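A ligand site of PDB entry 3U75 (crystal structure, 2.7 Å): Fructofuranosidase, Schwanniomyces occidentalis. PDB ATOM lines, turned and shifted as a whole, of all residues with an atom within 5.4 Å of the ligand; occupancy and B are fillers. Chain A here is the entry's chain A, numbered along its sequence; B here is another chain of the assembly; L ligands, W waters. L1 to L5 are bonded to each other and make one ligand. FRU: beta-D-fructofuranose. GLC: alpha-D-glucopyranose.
The guanidinium group (NH2) of Arg 178 sits at hydrogen-bond distance from an oxygen (O3) of FRU L2 (3.2 Å).
ND2 of Asn 49 sits at hydrogen-bond distance from O5 of FRU L1 (3.3 Å).
An oxygen (O6) of FRU L4 is in hydrogen-bond range of the backbone carbonyl oxygen (O) of Ser 434 of chain B (2.9 Å).
The backbone carbonyl oxygen (O) of Trp 76 lies close to an oxygen (O2) of GLC L5 (3.3 Å).
The indole nitrogen (NE1) of Trp 314 is in hydrogen-bond range of an oxygen (O1) of FRU L1, 2.8 Å away.
N of Trp 76 lies within hydrogen-bond range of O2 of GLC L5 (3.3 Å).
An oxygen (O4) of FRU L4 is in hydrogen-bond range of the backbone carbonyl oxygen (O) of Trp 314.
An oxygen (O3) of FRU L3 is in hydrogen-bond range of the side-chain amide nitrogen of Asn 254, 2.7 Å away.
O4 of FRU L4 is in hydrogen-bond range of OE1 of Gln 435 of chain B, at 2.8 Å.
N of Ser 111 is in hydrogen-bond range of O4 of FRU L1 (2.7 Å).
The side-chain amide nitrogen of Gln 68 sits at hydrogen-bond distance from an oxygen (O6) of FRU L1, 3.2 Å away.
O6 of FRU L1 lies within hydrogen-bond range of NE1 of Trp 76 (2.4 Å).
The side-chain amide oxygen (OE1) of Gln 228 is in hydrogen-bond range of an oxygen (O3) of FRU L2, 3.3 Å away.
An oxygen (O3) of FRU L1 sits at hydrogen-bond distance from the side-chain carboxylate (OD2) of Asp 179, at 2.6 Å.
An oxygen (O1) of FRU L1 lies close to the side-chain carboxylate (OD1) of Asp 50 (3.2 Å).
An oxygen (O3) of FRU L4 is in hydrogen-bond range of the side-chain carboxylate (OD1) of Asp 318, 2.8 Å away.
Ala 75 touches the ligand.
CD2 of Leu 80 touches O6 of FRU L1, at 3.5 Å.
CB of Phe 110 touches O4 of FRU L1, 3.4 Å away.
CD of Pro 255 touches O4 of FRU L3, 3.9 Å away.
CE2 of Tyr 293 touches O1 of FRU L1, at 3.0 Å.
NH1 of Arg 451 touches O4 of FRU L4 (3.5 Å).
Hydrophobic or aromatic side chains within 4 Å of the ligand: Ala 75, Trp 76, Leu 80, Phe 110, Pro 255, Tyr 293 and Trp 314.
19 residues have an atom within 4 Å of the ligand: Asn 49, Asp 50, Gln 68, Ala 75, Trp 76, Leu 80, Phe 110, Ser 111, Arg 178, Asp 179, Gln 228, Asn 254, Pro 255, Tyr 293, Trp 314, Asp 318, Arg 451, Ser 434 of chain B and Gln 435 of chain B.
The side-chain hydroxyl (OG) of Ser 434 of chain B sits at hydrogen-bond distance from the guanidinium group (NE) of Arg 451, at 3.2 Å.
The backbone NH (N) of Ser 111 sits at hydrogen-bond distance from the side-chain amide oxygen (OE1) of Gln 68, at 3.2 Å.
The side-chain amide oxygen of Gln 68 lies close to the backbone carbonyl oxygen of Phe 110 (2.8 Å).
The side-chain amide oxygen (OE1) of Gln 435 of chain B lies within hydrogen-bond range of the side-chain hydroxyl (OG) of Ser 434 of chain B (3.3 Å).
The side-chain amide oxygen (OE1) of Gln 176 lies within hydrogen-bond range of the guanidinium group (NH1) of Arg 178.
The side-chain carboxylate (OD2) of Asp 50 lies close to the side-chain hydroxyl (OG) of Ser 111 (3.2 Å).
The backbone carbonyl oxygen of Asp 50 sits at hydrogen-bond distance from the backbone NH of Gln 68 (2.9 Å).
The backbone NH (N) of Asn 49 lies within hydrogen-bond range of the backbone carbonyl oxygen (O) of Gln 68, at 3.0 Å.
Water W1 bridges the backbone carbonyl oxygen (O) of Gln 435 of chain B (3.4 Å) and an oxygen (O4) of FRU L3 (3.4 Å).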
ATOM      1  N   TRP A  47      -3.671  28.558 -23.642  1.00  0.00           N
ATOM      2  CA  TRP A  47      -4.849  28.414 -24.471  1.00  0.00           C
ATOM      3  C   TRP A  47      -5.992  29.309 -24.010  1.00  0.00           C
ATOM      4  O   TRP A  47      -6.403  29.240 -22.858  1.00  0.00           O
ATOM      5  CB  TRP A  47      -5.325  26.972 -24.436  1.00  0.00           C
ATOM      6  CG  TRP A  47      -6.664  26.854 -25.057  1.00  0.00           C
ATOM      7  CD1 TRP A  47      -7.874  27.008 -24.441  1.00  0.00           C
ATOM      8  CD2 TRP A  47      -6.933  26.626 -26.430  1.00  0.00           C
ATOM      9  NE1 TRP A  47      -8.881  26.873 -25.356  1.00  0.00           N
ATOM     10  CE2 TRP A  47      -8.343  26.636 -26.586  1.00  0.00           C
ATOM     11  CE3 TRP A  47      -6.123  26.405 -27.556  1.00  0.00           C
ATOM     12  CZ2 TRP A  47      -8.963  26.425 -27.813  1.00  0.00           C
ATOM     13  CZ3 TRP A  47      -6.736  26.198 -28.794  1.00  0.00           C
ATOM     14  CH2 TRP A  47      -8.159  26.200 -28.902  1.00  0.00           C
ATOM     15  N   ASN A  49      -9.998  30.502 -25.062  1.00  0.00           N
ATOM     16  CA  ASN A  49     -11.197  30.574 -25.890  1.00  0.00           C
ATOM     17  C   ASN A  49     -12.161  31.643 -25.385  1.00  0.00           C
ATOM     18  O   ASN A  49     -11.777  32.785 -25.217  1.00  0.00           O
ATOM     19  CB  ASN A  49     -11.848  29.188 -26.150  1.00  0.00           C
ATOM     20  CG  ASN A  49     -12.075  28.351 -24.885  1.00  0.00           C
ATOM     21  OD1 ASN A  49     -11.133  27.765 -24.330  1.00  0.00           O
ATOM     22  ND2 ASN A  49     -13.323  28.227 -24.482  1.00  0.00           N
ATOM     23  N   ASP A  50     -13.404  31.291 -25.127  1.00  0.00           N
ATOM     24  CA  ASP A  50     -14.448  32.266 -24.748  1.00  0.00           C
ATOM     25  C   ASP A  50     -13.990  33.426 -23.860  1.00  0.00           C
ATOM     26  O   ASP A  50     -13.390  33.206 -22.814  1.00  0.00           O
ATOM     27  CB  ASP A  50     -15.579  31.556 -24.027  1.00  0.00           C
ATOM     28  CG  ASP A  50     -16.319  30.603 -24.911  1.00  0.00           C
ATOM     29  OD1 ASP A  50     -15.665  29.838 -25.649  1.00  0.00           O
ATOM     30  OD2 ASP A  50     -17.549  30.620 -24.872  1.00  0.00           O
ATOM     31  N   GLN A  68     -11.591  31.899 -20.930  1.00  0.00           N
ATOM     32  CA  GLN A  68     -11.350  30.508 -20.768  1.00  0.00           C
ATOM     33  C   GLN A  68      -9.861  30.220 -21.014  1.00  0.00           C
ATOM     34  O   GLN A  68      -9.308  30.442 -22.106  1.00  0.00           O
ATOM     35  CB  GLN A  68     -12.263  29.725 -21.699  1.00  0.00           C
ATOM     36  CG  GLN A  68     -13.760  30.093 -21.480  1.00  0.00           C
ATOM     37  CD  GLN A  68     -14.284  29.540 -20.153  1.00  0.00           C
ATOM     38  OE1 GLN A  68     -14.473  30.277 -19.207  1.00  0.00           O
ATOM     39  NE2 GLN A  68     -14.490  28.233 -20.082  1.00  0.00           N
ATOM     40  N   ALA A  75      -3.687  23.805 -25.949  1.00  0.00           N
ATOM     41  CA  ALA A  75      -5.001  23.244 -26.332  1.00  0.00           C
ATOM     42  C   ALA A  75      -5.921  23.213 -25.103  1.00  0.00           C
ATOM     43  O   ALA A  75      -5.410  23.286 -23.990  1.00  0.00           O
ATOM     44  CB  ALA A  75      -4.835  21.835 -26.866  1.00  0.00           C
ATOM     45  N   TRP A  76      -7.242  23.093 -25.291  1.00  0.00           N
ATOM     46  CA  TRP A  76      -8.239  23.164 -24.206  1.00  0.00           C
ATOM     47  C   TRP A  76      -8.120  21.954 -23.317  1.00  0.00           C
ATOM     48  O   TRP A  76      -8.194  20.814 -23.808  1.00  0.00           O
ATOM     49  CB  TRP A  76      -9.640  23.209 -24.813  1.00  0.00           C
ATOM     50  CG  TRP A  76     -10.812  23.416 -23.850  1.00  0.00           C
ATOM     51  CD1 TRP A  76     -11.513  24.584 -23.661  1.00  0.00           C
ATOM     52  CD2 TRP A  76     -11.452  22.433 -23.011  1.00  0.00           C
ATOM     53  NE1 TRP A  76     -12.522  24.390 -22.756  1.00  0.00           N
ATOM     54  CE2 TRP A  76     -12.508  23.085 -22.341  1.00  0.00           C
ATOM     55  CE3 TRP A  76     -11.239  21.067 -22.790  1.00  0.00           C
ATOM     56  CZ2 TRP A  76     -13.363  22.420 -21.431  1.00  0.00           C
ATOM     57  CZ3 TRP A  76     -12.064  20.397 -21.883  1.00  0.00           C
ATOM     58  CH2 TRP A  76     -13.130  21.084 -21.214  1.00  0.00           C
ATOM     59  N   GLY A  77      -7.940  22.182 -22.028  1.00  0.00           N
ATOM     60  CA  GLY A  77      -7.870  21.107 -21.039  1.00  0.00           C
ATOM     61  C   GLY A  77      -8.211  21.575 -19.647  1.00  0.00           C
ATOM     62  O   GLY A  77      -8.115  22.744 -19.341  1.00  0.00           O
ATOM     63  N   LEU A  80      -9.514  24.156 -15.707  1.00  0.00           N
ATOM     64  CA  LEU A  80      -9.786  25.264 -16.588  1.00  0.00           C
ATOM     65  C   LEU A  80     -10.212  26.488 -15.797  1.00  0.00           C
ATOM     66  O   LEU A  80     -11.152  26.414 -14.976  1.00  0.00           O
ATOM     67  CB  LEU A  80     -10.877  24.879 -17.600  1.00  0.00           C
ATOM     68  CG  LEU A  80     -11.255  25.927 -18.649  1.00  0.00           C
ATOM     69  CD1 LEU A  80     -10.343  25.793 -19.877  1.00  0.00           C
ATOM     70  CD2 LEU A  80     -12.731  25.847 -19.029  1.00  0.00           C
ATOM     71  N   PHE A 110     -16.069  27.300 -16.330  1.00  0.00           N
ATOM     72  CA  PHE A 110     -16.509  27.531 -17.696  1.00  0.00           C
ATOM     73  C   PHE A 110     -16.864  29.003 -18.009  1.00  0.00           C
ATOM     74  O   PHE A 110     -16.501  29.902 -17.267  1.00  0.00           O
ATOM     75  CB  PHE A 110     -17.611  26.539 -18.040  1.00  0.00           C
ATOM     76  CG  PHE A 110     -17.085  25.217 -18.528  1.00  0.00           C
ATOM     77  CD1 PHE A 110     -15.834  24.752 -18.104  1.00  0.00           C
ATOM     78  CD2 PHE A 110     -17.822  24.448 -19.401  1.00  0.00           C
ATOM     79  CE1 PHE A 110     -15.340  23.531 -18.550  1.00  0.00           C
ATOM     80  CE2 PHE A 110     -17.328  23.227 -19.847  1.00  0.00           C
ATOM     81  CZ  PHE A 110     -16.099  22.766 -19.424  1.00  0.00           C
ATOM     82  N   SER A 111     -17.514  29.253 -19.127  1.00  0.00           N
ATOM     83  CA  SER A 111     -17.861  30.621 -19.462  1.00  0.00           C
ATOM     84  C   SER A 111     -18.880  31.223 -18.463  1.00  0.00           C
ATOM     85  O   SER A 111     -19.458  30.533 -17.639  1.00  0.00           O
ATOM     86  CB  SER A 111     -18.363  30.700 -20.907  1.00  0.00           C
ATOM     87  OG  SER A 111     -17.348  31.214 -21.731  1.00  0.00           O
ATOM     88  N   GLN A 147     -23.038  20.339 -14.364  1.00  0.00           N
ATOM     89  CA  GLN A 147     -22.771  21.729 -14.762  1.00  0.00           C
ATOM     90  C   GLN A 147     -23.776  22.652 -14.079  1.00  0.00           C
ATOM     91  O   GLN A 147     -24.997  22.506 -14.259  1.00  0.00           O
ATOM     92  CB  GLN A 147     -22.812  21.915 -16.284  1.00  0.00           C
ATOM     93  CG  GLN A 147     -21.580  21.371 -17.015  1.00  0.00           C
ATOM     94  CD  GLN A 147     -21.546  21.704 -18.503  1.00  0.00           C
ATOM     95  OE1 GLN A 147     -22.450  22.356 -19.026  1.00  0.00           O
ATOM     96  NE2 GLN A 147     -20.476  21.279 -19.192  1.00  0.00           N
ATOM     97  N   GLN A 176     -25.518  19.522 -19.327  1.00  0.00           N
ATOM     98  CA  GLN A 176     -25.455  20.459 -20.477  1.00  0.00           C
ATOM     99  C   GLN A 176     -26.265  21.722 -20.194  1.00  0.00           C
ATOM    100  O   GLN A 176     -27.419  21.874 -20.664  1.00  0.00           O
ATOM    101  CB  GLN A 176     -25.996  19.805 -21.749  1.00  0.00           C
ATOM    102  CG  GLN A 176     -25.261  18.537 -22.159  1.00  0.00           C
ATOM    103  CD  GLN A 176     -23.954  18.805 -22.904  1.00  0.00           C
ATOM    104  OE1 GLN A 176     -23.761  19.850 -23.547  1.00  0.00           O
ATOM    105  NE2 GLN A 176     -23.057  17.835 -22.853  1.00  0.00           N
ATOM    106  N   ARG A 178     -24.956  25.722 -19.276  1.00  0.00           N
ATOM    107  CA  ARG A 178     -23.759  26.544 -19.153  1.00  0.00           C
ATOM    108  C   ARG A 178     -23.858  27.902 -19.829  1.00  0.00           C
ATOM    109  O   ARG A 178     -24.670  28.084 -20.728  1.00  0.00           O
ATOM    110  CB  ARG A 178     -22.548  25.769 -19.697  1.00  0.00           C
ATOM    111  CG  ARG A 178     -22.761  25.200 -21.079  1.00  0.00           C
ATOM    112  CD  ARG A 178     -21.492  24.724 -21.753  1.00  0.00           C
ATOM    113  NE  ARG A 178     -21.783  24.199 -23.093  1.00  0.00           N
ATOM    114  CZ  ARG A 178     -22.176  22.951 -23.372  1.00  0.00           C
ATOM    115  NH1 ARG A 178     -22.329  22.030 -22.441  1.00  0.00           N
ATOM    116  NH2 ARG A 178     -22.419  22.619 -24.618  1.00  0.00           N
ATOM    117  N   ASP A 179     -23.018  28.840 -19.350  1.00  0.00           N
ATOM    118  CA  ASP A 179     -22.678  30.135 -19.981  1.00  0.00           C
ATOM    119  C   ASP A 179     -23.709  31.234 -19.769  1.00  0.00           C
ATOM    120  O   ASP A 179     -24.415  31.603 -20.696  1.00  0.00           O
ATOM    121  CB  ASP A 179     -22.346  30.017 -21.485  1.00  0.00           C
ATOM    122  CG  ASP A 179     -21.808  28.645 -21.861  1.00  0.00           C
ATOM    123  OD1 ASP A 179     -21.139  27.996 -21.016  1.00  0.00           O
ATOM    124  OD2 ASP A 179     -22.090  28.201 -23.006  1.00  0.00           O
ATOM    125  N   GLN A 228     -25.567  22.767 -30.953  1.00  0.00           N
ATOM    126  CA  GLN A 228     -25.592  23.299 -29.593  1.00  0.00           C
ATOM    127  C   GLN A 228     -25.747  24.799 -29.612  1.00  0.00           C
ATOM    128  O   GLN A 228     -25.020  25.504 -30.367  1.00  0.00           O
ATOM    129  CB  GLN A 228     -24.272  23.068 -28.872  1.00  0.00           C
ATOM    130  CG  GLN A 228     -24.206  21.916 -27.909  1.00  0.00           C
ATOM    131  CD  GLN A 228     -22.760  21.509 -27.674  1.00  0.00           C
ATOM    132  OE1 GLN A 228     -21.849  22.018 -28.329  1.00  0.00           O
ATOM    133  NE2 GLN A 228     -22.539  20.574 -26.754  1.00  0.00           N
ATOM    134  N   ALA A 230     -25.085  28.094 -27.255  1.00  0.00           N
ATOM    135  CA  ALA A 230     -24.003  28.469 -26.292  1.00  0.00           C
ATOM    136  C   ALA A 230     -23.820  29.980 -26.128  1.00  0.00           C
ATOM    137  O   ALA A 230     -24.108  30.734 -27.032  1.00  0.00           O
ATOM    138  CB  ALA A 230     -22.662  27.815 -26.669  1.00  0.00           C
ATOM    139  N   CYS A 231     -23.314  30.399 -24.964  1.00  0.00           N
ATOM    140  CA  CYS A 231     -22.930  31.797 -24.747  1.00  0.00           C
ATOM    141  C   CYS A 231     -23.949  32.799 -25.246  1.00  0.00           C
ATOM    142  O   CYS A 231     -23.610  33.641 -26.064  1.00  0.00           O
ATOM    143  CB  CYS A 231     -21.634  32.080 -25.467  1.00  0.00           C
ATOM    144  SG  CYS A 231     -20.329  31.006 -24.975  1.00  0.00           S
ATOM    145  N   ASN A 254     -21.900  25.984 -31.989  1.00  0.00           N
ATOM    146  CA  ASN A 254     -20.857  25.103 -32.379  1.00  0.00           C
ATOM    147  C   ASN A 254     -21.101  23.671 -31.893  1.00  0.00           C
ATOM    148  O   ASN A 254     -21.651  23.457 -30.822  1.00  0.00           O
ATOM    149  CB  ASN A 254     -19.552  25.628 -31.832  1.00  0.00           C
ATOM    150  CG  ASN A 254     -18.420  24.690 -32.108  1.00  0.00           C
ATOM    151  OD1 ASN A 254     -17.908  24.626 -33.238  1.00  0.00           O
ATOM    152  ND2 ASN A 254     -18.018  23.949 -31.088  1.00  0.00           N
ATOM    153  N   PRO A 255     -20.724  22.662 -32.721  1.00  0.00           N
ATOM    154  CA  PRO A 255     -20.386  22.793 -34.134  1.00  0.00           C
ATOM    155  C   PRO A 255     -21.624  22.941 -35.038  1.00  0.00           C
ATOM    156  O   PRO A 255     -22.759  23.147 -34.533  1.00  0.00           O
ATOM    157  CB  PRO A 255     -19.645  21.492 -34.421  1.00  0.00           C
ATOM    158  CG  PRO A 255     -20.189  20.559 -33.438  1.00  0.00           C
ATOM    159  CD  PRO A 255     -20.378  21.331 -32.211  1.00  0.00           C
ATOM    160  N   TYR A 293     -16.480  33.717 -32.635  1.00  0.00           N
ATOM    161  CA  TYR A 293     -17.336  32.889 -31.785  1.00  0.00           C
ATOM    162  C   TYR A 293     -17.300  33.412 -30.382  1.00  0.00           C
ATOM    163  O   TYR A 293     -16.292  33.967 -29.954  1.00  0.00           O
ATOM    164  CB  TYR A 293     -16.854  31.427 -31.767  1.00  0.00           C
ATOM    165  CG  TYR A 293     -17.764  30.414 -31.052  1.00  0.00           C
ATOM    166  CD1 TYR A 293     -18.993  30.057 -31.590  1.00  0.00           C
ATOM    167  CD2 TYR A 293     -17.370  29.799 -29.856  1.00  0.00           C
ATOM    168  CE1 TYR A 293     -19.815  29.128 -30.962  1.00  0.00           C
ATOM    169  CE2 TYR A 293     -18.193  28.848 -29.202  1.00  0.00           C
ATOM    170  CZ  TYR A 293     -19.419  28.522 -29.762  1.00  0.00           C
ATOM    171  OH  TYR A 293     -20.244  27.597 -29.141  1.00  0.00           O
ATOM    172  N   ALA A 294     -18.400  33.198 -29.667  1.00  0.00           N
ATOM    173  CA  ALA A 294     -18.490  33.466 -28.251  1.00  0.00           C
ATOM    174  C   ALA A 294     -18.347  34.947 -27.945  1.00  0.00           C
ATOM    175  O   ALA A 294     -17.631  35.347 -27.028  1.00  0.00           O
ATOM    176  CB  ALA A 294     -17.485  32.656 -27.492  1.00  0.00           C
ATOM    177  N   TRP A 314     -13.665  26.548 -33.789  1.00  0.00           N
ATOM    178  CA  TRP A 314     -13.436  25.298 -33.072  1.00  0.00           C
ATOM    179  C   TRP A 314     -13.000  24.120 -33.974  1.00  0.00           C
ATOM    180  O   TRP A 314     -12.495  23.104 -33.507  1.00  0.00           O
ATOM    181  CB  TRP A 314     -14.655  24.926 -32.236  1.00  0.00           C
ATOM    182  CG  TRP A 314     -14.751  25.586 -30.877  1.00  0.00           C
ATOM    183  CD1 TRP A 314     -15.663  26.516 -30.490  1.00  0.00           C
ATOM    184  CD2 TRP A 314     -13.948  25.322 -29.731  1.00  0.00           C
ATOM    185  NE1 TRP A 314     -15.474  26.860 -29.168  1.00  0.00           N
ATOM    186  CE2 TRP A 314     -14.426  26.135 -28.680  1.00  0.00           C
ATOM    187  CE3 TRP A 314     -12.850  24.485 -29.475  1.00  0.00           C
ATOM    188  CZ2 TRP A 314     -13.851  26.147 -27.408  1.00  0.00           C
ATOM    189  CZ3 TRP A 314     -12.277  24.511 -28.208  1.00  0.00           C
ATOM    190  CH2 TRP A 314     -12.782  25.336 -27.199  1.00  0.00           C
ATOM    191  N   GLN A 315     -13.202  24.259 -35.278  1.00  0.00           N
ATOM    192  CA  GLN A 315     -12.701  23.253 -36.201  1.00  0.00           C
ATOM    193  C   GLN A 315     -11.167  23.104 -36.225  1.00  0.00           C
ATOM    194  O   GLN A 315     -10.644  22.019 -36.433  1.00  0.00           O
ATOM    195  CB  GLN A 315     -13.236  23.549 -37.591  1.00  0.00           C
ATOM    196  CG  GLN A 315     -14.563  22.901 -37.943  1.00  0.00           C
ATOM    197  CD  GLN A 315     -15.143  23.375 -39.282  1.00  0.00           C
ATOM    198  OE1 GLN A 315     -14.999  24.541 -39.640  1.00  0.00           O
ATOM    199  NE2 GLN A 315     -15.812  22.469 -40.003  1.00  0.00           N
ATOM    200  N   ASP A 318      -7.089  24.577 -32.182  1.00  0.00           N
ATOM    201  CA  ASP A 318      -5.970  23.981 -31.463  1.00  0.00           C
ATOM    202  C   ASP A 318      -4.871  23.437 -32.381  1.00  0.00           C
ATOM    203  O   ASP A 318      -3.933  22.809 -31.906  1.00  0.00           O
ATOM    204  CB  ASP A 318      -6.411  22.958 -30.377  1.00  0.00           C
ATOM    205  CG  ASP A 318      -7.178  21.747 -30.908  1.00  0.00           C
ATOM    206  OD1 ASP A 318      -7.654  20.901 -30.110  1.00  0.00           O
ATOM    207  OD2 ASP A 318      -7.313  21.601 -32.124  1.00  0.00           O
ATOM    208  N   ARG A 451      -6.127  19.590 -39.733  1.00  0.00           N
ATOM    209  CA  ARG A 451      -7.516  20.027 -39.914  1.00  0.00           C
ATOM    210  C   ARG A 451      -7.735  21.194 -40.857  1.00  0.00           C
ATOM    211  O   ARG A 451      -8.815  21.797 -40.835  1.00  0.00           O
ATOM    212  CB  ARG A 451      -8.225  20.256 -38.598  1.00  0.00           C
ATOM    213  CG  ARG A 451      -8.295  18.991 -37.819  1.00  0.00           C
ATOM    214  CD  ARG A 451      -9.444  19.005 -36.883  1.00  0.00           C
ATOM    215  NE  ARG A 451      -9.030  18.340 -35.660  1.00  0.00           N
ATOM    216  CZ  ARG A 451      -8.602  18.979 -34.578  1.00  0.00           C
ATOM    217  NH1 ARG A 451      -8.555  20.308 -34.538  1.00  0.00           N
ATOM    218  NH2 ARG A 451      -8.236  18.262 -33.543  1.00  0.00           N
ATOM    219  N   SER B 434     -12.409  13.123 -35.346  1.00  0.00           N
ATOM    220  CA  SER B 434     -12.334  14.108 -34.291  1.00  0.00           C
ATOM    221  C   SER B 434     -13.360  15.236 -34.459  1.00  0.00           C
ATOM    222  O   SER B 434     -13.581  15.992 -33.515  1.00  0.00           O
ATOM    223  CB  SER B 434     -10.950  14.706 -34.238  1.00  0.00           C
ATOM    224  OG  SER B 434     -10.874  15.742 -35.186  1.00  0.00           O
ATOM    225  N   GLN B 435     -13.950  15.348 -35.649  1.00  0.00           N
ATOM    226  CA  GLN B 435     -14.828  16.480 -35.958  1.00  0.00           C
ATOM    227  C   GLN B 435     -16.246  16.021 -36.211  1.00  0.00           C
ATOM    228  O   GLN B 435     -17.148  16.857 -36.258  1.00  0.00           O
ATOM    229  CB  GLN B 435     -14.335  17.238 -37.202  1.00  0.00           C
ATOM    230  CG  GLN B 435     -13.150  18.213 -37.018  1.00  0.00           C
ATOM    231  CD  GLN B 435     -13.199  18.964 -35.714  1.00  0.00           C
ATOM    232  OE1 GLN B 435     -12.415  18.690 -34.792  1.00  0.00           O
ATOM    233  NE2 GLN B 435     -14.130  19.908 -35.609  1.00  0.00           N
HETATM  234  C1  FRU L   1     -17.800  27.867 -25.785  1.00  0.00           C
HETATM  235  C2  FRU L   1     -17.602  26.973 -24.561  1.00  0.00           C
HETATM  236  C3  FRU L   1     -18.580  27.428 -23.499  1.00  0.00           C
HETATM  237  C4  FRU L   1     -18.038  26.841 -22.239  1.00  0.00           C
HETATM  238  C5  FRU L   1     -16.530  26.938 -22.459  1.00  0.00           C
HETATM  239  C6  FRU L   1     -15.831  25.655 -22.016  1.00  0.00           C
HETATM  240  O1  FRU L   1     -17.123  27.319 -26.909  1.00  0.00           O
HETATM  241  O3  FRU L   1     -19.880  27.012 -23.812  1.00  0.00           O
HETATM  242  O4  FRU L   1     -18.432  27.695 -21.175  1.00  0.00           O
HETATM  243  O5  FRU L   1     -16.349  27.182 -23.871  1.00  0.00           O
HETATM  244  O6  FRU L   1     -14.407  25.757 -22.045  1.00  0.00           O
HETATM  245  C1  FRU L   2     -16.834  24.610 -25.469  1.00  0.00           C
HETATM  246  C2  FRU L   2     -17.141  23.098 -25.514  1.00  0.00           C
HETATM  247  C3  FRU L   2     -18.573  22.785 -25.065  1.00  0.00           C
HETATM  248  C4  FRU L   2     -18.464  21.344 -24.615  1.00  0.00           C
HETATM  249  C5  FRU L   2     -17.074  21.313 -23.984  1.00  0.00           C
HETATM  250  C6  FRU L   2     -16.253  20.070 -24.320  1.00  0.00           C
HETATM  251  O1  FRU L   2     -17.813  25.570 -24.909  1.00  0.00           O
HETATM  252  O3  FRU L   2     -19.598  22.967 -26.059  1.00  0.00           O
HETATM  253  O4  FRU L   2     -19.494  21.013 -23.666  1.00  0.00           O
HETATM  254  O5  FRU L   2     -16.365  22.450 -24.520  1.00  0.00           O
HETATM  255  O6  FRU L   2     -14.901  20.501 -24.664  1.00  0.00           O
HETATM  256  C1  FRU L   3     -15.499  22.239 -27.070  1.00  0.00           C
HETATM  257  C2  FRU L   3     -15.302  21.246 -28.201  1.00  0.00           C
HETATM  258  C3  FRU L   3     -16.435  21.243 -29.225  1.00  0.00           C
HETATM  259  C4  FRU L   3     -16.425  19.806 -29.664  1.00  0.00           C
HETATM  260  C5  FRU L   3     -16.215  19.048 -28.374  1.00  0.00           C
HETATM  261  C6  FRU L   3     -15.685  17.639 -28.634  1.00  0.00           C
HETATM  262  O1  FRU L   3     -16.881  22.444 -26.767  1.00  0.00           O
HETATM  263  O3  FRU L   3     -16.239  22.062 -30.380  1.00  0.00           O
HETATM  264  O4  FRU L   3     -17.591  19.366 -30.353  1.00  0.00           O
HETATM  265  O5  FRU L   3     -15.297  19.918 -27.675  1.00  0.00           O
HETATM  266  O6  FRU L   3     -14.758  17.614 -29.763  1.00  0.00           O
HETATM  267  C1  FRU L   4     -12.903  21.152 -28.083  1.00  0.00           C
HETATM  268  C2  FRU L   4     -11.991  20.293 -28.971  1.00  0.00           C
HETATM  269  C3  FRU L   4     -11.492  20.960 -30.241  1.00  0.00           C
HETATM  270  C4  FRU L   4     -11.194  19.763 -31.158  1.00  0.00           C
HETATM  271  C5  FRU L   4     -12.105  18.660 -30.645  1.00  0.00           C
HETATM  272  C6  FRU L   4     -11.366  17.347 -30.388  1.00  0.00           C
HETATM  273  O1  FRU L   4     -14.047  21.525 -28.812  1.00  0.00           O
HETATM  274  O3  FRU L   4     -10.323  21.712 -29.916  1.00  0.00           O
HETATM  275  O4  FRU L   4     -11.460  20.024 -32.553  1.00  0.00           O
HETATM  276  O5  FRU L   4     -12.686  19.105 -29.410  1.00  0.00           O
HETATM  277  O6  FRU L   4     -12.056  16.330 -31.122  1.00  0.00           O
HETATM  278  C1  GLC L   5     -10.637  19.991 -26.915  1.00  0.00           C
HETATM  279  C2  GLC L   5      -9.202  19.552 -26.598  1.00  0.00           C
HETATM  280  C3  GLC L   5      -9.051  18.210 -27.306  1.00  0.00           C
HETATM  281  C4  GLC L   5      -9.953  17.187 -26.623  1.00  0.00           C
HETATM  282  C5  GLC L   5     -11.397  17.672 -26.448  1.00  0.00           C
HETATM  283  C6  GLC L   5     -11.972  17.012 -25.204  1.00  0.00           C
HETATM  284  O1  GLC L   5     -10.763  19.951 -28.330  1.00  0.00           O
HETATM  285  O2  GLC L   5      -8.275  20.507 -27.110  1.00  0.00           O
HETATM  286  O3  GLC L   5      -7.670  17.796 -27.407  1.00  0.00           O
HETATM  287  O4  GLC L   5     -10.037  16.003 -27.420  1.00  0.00           O
HETATM  288  O5  GLC L   5     -11.571  19.093 -26.298  1.00  0.00           O
HETATM  289  O6  GLC L   5     -13.316  16.678 -25.529  1.00  0.00           O
HETATM  290  O   HOH W   1     -17.226  17.082 -32.912  1.00  0.00           O
